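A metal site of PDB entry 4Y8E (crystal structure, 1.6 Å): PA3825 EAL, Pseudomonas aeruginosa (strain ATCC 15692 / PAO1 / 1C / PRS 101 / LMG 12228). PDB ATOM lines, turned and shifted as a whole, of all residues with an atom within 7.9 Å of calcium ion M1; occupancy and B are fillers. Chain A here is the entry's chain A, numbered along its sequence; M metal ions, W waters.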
ATOM      1  N   GLU A  39      -9.846 -29.317  -8.798  1.00  0.00           N
ATOM      2  CA  GLU A  39      -9.106 -28.105  -8.878  1.00  0.00           C
ATOM      3  C   GLU A  39      -9.302 -27.596 -10.281  1.00  0.00           C
ATOM      4  O   GLU A  39      -9.080 -28.301 -11.272  1.00  0.00           O
ATOM      5  CB  GLU A  39      -7.630 -28.319  -8.540  1.00  0.00           C
ATOM      6  CG  GLU A  39      -7.487 -28.818  -7.116  1.00  0.00           C
ATOM      7  CD  GLU A  39      -7.544 -27.676  -6.109  1.00  0.00           C
ATOM      8  OE1 GLU A  39      -7.990 -26.564  -6.517  1.00  0.00           O
ATOM      9  OE2 GLU A  39      -7.180 -27.836  -4.956  1.00  0.00           O
ATOM     10  N   ASN A  98      -7.349 -21.153  -8.022  1.00  0.00           N
ATOM     11  CA  ASN A  98      -6.124 -20.471  -7.654  1.00  0.00           C
ATOM     12  C   ASN A  98      -6.412 -18.952  -7.783  1.00  0.00           C
ATOM     13  O   ASN A  98      -6.651 -18.475  -8.929  1.00  0.00           O
ATOM     14  CB  ASN A  98      -5.077 -20.851  -8.634  1.00  0.00           C
ATOM     15  CG  ASN A  98      -3.717 -20.205  -8.332  1.00  0.00           C
ATOM     16  OD1 ASN A  98      -3.620 -19.104  -7.802  1.00  0.00           O
ATOM     17  ND2 ASN A  98      -2.628 -20.897  -8.733  1.00  0.00           N
ATOM     18  N   GLU A 130      -7.802 -20.697  -3.170  1.00  0.00           N
ATOM     19  CA  GLU A 130      -6.450 -21.064  -2.789  1.00  0.00           C
ATOM     20  C   GLU A 130      -5.475 -19.889  -3.007  1.00  0.00           C
ATOM     21  O   GLU A 130      -5.363 -19.425  -4.139  1.00  0.00           O
ATOM     22  CB  GLU A 130      -6.047 -22.322  -3.658  1.00  0.00           C
ATOM     23  CG  GLU A 130      -7.115 -23.423  -3.514  1.00  0.00           C
ATOM     24  CD  GLU A 130      -6.767 -24.787  -4.092  1.00  0.00           C
ATOM     25  OE1 GLU A 130      -5.868 -24.887  -4.908  1.00  0.00           O
ATOM     26  OE2 GLU A 130      -7.494 -25.756  -3.664  1.00  0.00           O
ATOM     27  N   THR A 132      -1.437 -18.558  -1.941  1.00  0.00           N
ATOM     28  CA  THR A 132      -0.128 -18.821  -1.347  1.00  0.00           C
ATOM     29  C   THR A 132       0.193 -18.017  -0.133  1.00  0.00           C
ATOM     30  O   THR A 132      -0.452 -16.992   0.166  1.00  0.00           O
ATOM     31  CB  THR A 132       0.968 -18.665  -2.384  1.00  0.00           C
ATOM     32  OG1 THR A 132       1.083 -17.254  -2.711  1.00  0.00           O
ATOM     33  CG2 THR A 132       0.772 -19.440  -3.631  1.00  0.00           C
ATOM     34  N   ILE A 159      -4.325 -22.636   1.992  1.00  0.00           N
ATOM     35  CA  ILE A 159      -3.034 -22.120   1.749  1.00  0.00           C
ATOM     36  C   ILE A 159      -2.397 -22.922   0.690  1.00  0.00           C
ATOM     37  O   ILE A 159      -2.019 -24.126   0.950  1.00  0.00           O
ATOM     38  CB  ILE A 159      -2.145 -22.060   3.031  1.00  0.00           C
ATOM     39  CG1 ILE A 159      -2.901 -21.264   4.125  1.00  0.00           C
ATOM     40  CG2 ILE A 159      -0.841 -21.407   2.717  1.00  0.00           C
ATOM     41  CD1 ILE A 159      -2.123 -21.026   5.432  1.00  0.00           C
ATOM     42  N   ASP A 160      -2.153 -22.338  -0.453  1.00  0.00           N
ATOM     43  CA  ASP A 160      -1.624 -23.027  -1.613  1.00  0.00           C
ATOM     44  C   ASP A 160      -0.130 -23.172  -1.547  1.00  0.00           C
ATOM     45  O   ASP A 160       0.607 -22.351  -0.948  1.00  0.00           O
ATOM     46  CB  ASP A 160      -2.047 -22.197  -2.800  1.00  0.00           C
ATOM     47  CG  ASP A 160      -1.882 -22.863  -4.110  1.00  0.00           C
ATOM     48  OD1 ASP A 160      -1.541 -24.133  -4.200  1.00  0.00           O
ATOM     49  OD2 ASP A 160      -2.098 -22.237  -5.180  1.00  0.00           O
ATOM     50  N   ASP A 161       0.386 -24.305  -2.016  1.00  0.00           N
ATOM     51  CA  ASP A 161       1.831 -24.572  -1.949  1.00  0.00           C
ATOM     52  C   ASP A 161       2.492 -24.345  -0.578  1.00  0.00           C
ATOM     53  O   ASP A 161       3.583 -23.735  -0.474  1.00  0.00           O
ATOM     54  CB  ASP A 161       2.571 -23.800  -3.026  1.00  0.00           C
ATOM     55  CG  ASP A 161       2.018 -24.066  -4.392  1.00  0.00           C
ATOM     56  OD1 ASP A 161       1.269 -25.081  -4.656  1.00  0.00           O
ATOM     57  OD2 ASP A 161       2.281 -23.183  -5.269  1.00  0.00           O
ATOM     58  N   PHE A 162       1.856 -24.844   0.468  1.00  0.00           N
ATOM     59  CA  PHE A 162       2.321 -24.617   1.803  1.00  0.00           C
ATOM     60  C   PHE A 162       3.741 -25.261   2.014  1.00  0.00           C
ATOM     61  O   PHE A 162       3.976 -26.371   1.530  1.00  0.00           O
ATOM     62  CB  PHE A 162       1.407 -25.219   2.784  1.00  0.00           C
ATOM     63  CG  PHE A 162       1.778 -24.908   4.203  1.00  0.00           C
ATOM     64  CD1 PHE A 162       1.475 -23.696   4.738  1.00  0.00           C
ATOM     65  CD2 PHE A 162       2.518 -25.809   4.962  1.00  0.00           C
ATOM     66  CE1 PHE A 162       1.828 -23.369   6.025  1.00  0.00           C
ATOM     67  CE2 PHE A 162       2.875 -25.508   6.268  1.00  0.00           C
ATOM     68  CZ  PHE A 162       2.539 -24.274   6.815  1.00  0.00           C
ATOM     69  N   LYS A 181      -2.414 -26.844   1.752  1.00  0.00           N
ATOM     70  CA  LYS A 181      -2.054 -27.690   0.622  1.00  0.00           C
ATOM     71  C   LYS A 181      -0.576 -27.949   0.682  1.00  0.00           C
ATOM     72  O   LYS A 181       0.277 -27.054   0.457  1.00  0.00           O
ATOM     73  CB  LYS A 181      -2.418 -27.103  -0.709  1.00  0.00           C
ATOM     74  CG  LYS A 181      -3.826 -26.595  -0.815  1.00  0.00           C
ATOM     75  CD  LYS A 181      -4.310 -26.362  -2.204  1.00  0.00           C
ATOM     76  CE  LYS A 181      -4.462 -27.671  -3.036  1.00  0.00           C
ATOM     77  NZ  LYS A 181      -4.495 -27.371  -4.479  1.00  0.00           N
ATOM     78  N   ILE A 182      -0.167 -29.186   0.877  1.00  0.00           N
ATOM     79  CA  ILE A 182       1.217 -29.496   0.975  1.00  0.00           C
ATOM     80  C   ILE A 182       1.879 -29.375  -0.385  1.00  0.00           C
ATOM     81  O   ILE A 182       1.464 -30.005  -1.354  1.00  0.00           O
ATOM     82  CB  ILE A 182       1.449 -30.978   1.469  1.00  0.00           C
ATOM     83  CG1 ILE A 182       0.814 -31.268   2.826  1.00  0.00           C
ATOM     84  CG2 ILE A 182       2.928 -31.288   1.530  1.00  0.00           C
ATOM     85  CD1 ILE A 182       0.622 -32.760   3.126  1.00  0.00           C
ATOM     86  N   ASP A 183       2.929 -28.557  -0.538  1.00  0.00           N
ATOM     87  CA  ASP A 183       3.646 -28.398  -1.762  1.00  0.00           C
ATOM     88  C   ASP A 183       4.156 -29.727  -2.309  1.00  0.00           C
ATOM     89  O   ASP A 183       4.634 -30.589  -1.516  1.00  0.00           O
ATOM     90  CB  ASP A 183       4.834 -27.426  -1.622  1.00  0.00           C
ATOM     91  CG  ASP A 183       5.358 -27.016  -2.963  1.00  0.00           C
ATOM     92  OD1 ASP A 183       4.591 -26.296  -3.682  1.00  0.00           O
ATOM     93  OD2 ASP A 183       6.461 -27.505  -3.325  1.00  0.00           O
ATOM     94  N   GLN A 184       4.118 -29.882  -3.633  1.00  0.00           N
ATOM     95  CA  GLN A 184       4.590 -31.110  -4.276  1.00  0.00           C
ATOM     96  C   GLN A 184       6.048 -31.480  -3.913  1.00  0.00           C
ATOM     97  O   GLN A 184       6.403 -32.668  -3.897  1.00  0.00           O
ATOM     98  CB  GLN A 184       4.450 -30.987  -5.773  1.00  0.00           C
ATOM     99  CG  GLN A 184       5.336 -29.921  -6.464  1.00  0.00           C
ATOM    100  CD  GLN A 184       6.771 -30.391  -6.687  1.00  0.00           C
ATOM    101  OE1 GLN A 184       7.027 -31.610  -6.897  1.00  0.00           O
ATOM    102  NE2 GLN A 184       7.692 -29.430  -6.711  1.00  0.00           N
ATOM    103  N   GLU A 217      -0.315 -32.143  -2.713  1.00  0.00           N
ATOM    104  CA  GLU A 217      -0.120 -31.945  -4.136  1.00  0.00           C
ATOM    105  C   GLU A 217       0.974 -32.792  -4.696  1.00  0.00           C
ATOM    106  O   GLU A 217       1.870 -33.260  -3.969  1.00  0.00           O
ATOM    107  CB  GLU A 217       0.164 -30.480  -4.403  1.00  0.00           C
ATOM    108  CG  GLU A 217      -0.896 -29.495  -3.993  1.00  0.00           C
ATOM    109  CD  GLU A 217      -0.684 -28.067  -4.568  1.00  0.00           C
ATOM    110  OE1 GLU A 217       0.109 -27.835  -5.485  1.00  0.00           O
ATOM    111  OE2 GLU A 217      -1.509 -27.282  -4.216  1.00  0.00           O
ATOM    112  N   GLY A 218       0.971 -33.068  -5.988  1.00  0.00           N
ATOM    113  CA  GLY A 218       2.008 -33.869  -6.535  1.00  0.00           C
ATOM    114  C   GLY A 218       2.067 -35.346  -6.202  1.00  0.00           C
ATOM    115  O   GLY A 218       3.184 -35.919  -6.204  1.00  0.00           O
ATOM    116  N   GLN A 237      -4.073 -34.888  -4.664  1.00  0.00           N
ATOM    117  CA  GLN A 237      -4.068 -34.481  -6.062  1.00  0.00           C
ATOM    118  C   GLN A 237      -2.710 -34.747  -6.693  1.00  0.00           C
ATOM    119  O   GLN A 237      -1.683 -34.695  -6.015  1.00  0.00           O
ATOM    120  CB  GLN A 237      -4.514 -33.017  -6.320  1.00  0.00           C
ATOM    121  CG  GLN A 237      -3.624 -32.030  -5.782  1.00  0.00           C
ATOM    122  CD  GLN A 237      -3.983 -30.574  -6.184  1.00  0.00           C
ATOM    123  OE1 GLN A 237      -3.522 -30.028  -7.170  1.00  0.00           O
ATOM    124  NE2 GLN A 237      -4.815 -30.062  -5.477  1.00  0.00           N
HETATM  125 CA    CA M   1      -0.643 -25.605  -5.835  1.00  0.00          CA
HETATM  126 CA    CA M   2      -0.807 -31.697  -8.292  1.00  0.00          CA
HETATM  127  O   HOH W   1      -0.748 -23.576  -6.993  1.00  0.00           O
HETATM  128  O   HOH W   2      -2.941 -25.943  -6.553  1.00  0.00           O
HETATM  129  O   HOH W   3       0.390 -26.239  -7.812  1.00  0.00           O
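The side-chain amino group (NZ) of Lys 181 sits close to the side-chain carboxylate (OE2) of Glu 217. N of Glu 217 lies within hydrogen-bond range of O of Ile 182, at 3.1 Å.
Three residues have an atom within 4 Å of calcium ion M1: Asp 160, Asp 161 and Glu 217. The nearest printed residue that does not touch calcium ion M1 is Lys 181 (4.4 Å).
OD1 of Asp 161 binds calcium ion M1 (2.3 Å). Calcium ion M1 is bound by water W3 (2.3 Å). Calcium ion M1 is bound by water W1. The side-chain carboxylate (OD1) of Asp 160 binds calcium ion M1, 2.4 Å away. OE1 of Glu 217 is bound to calcium ion M1. Calcium ion M1 is bound by water W2, at 2.4 Å. OE2 of Glu 217 binds calcium ion M1, at 2.5 Å.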
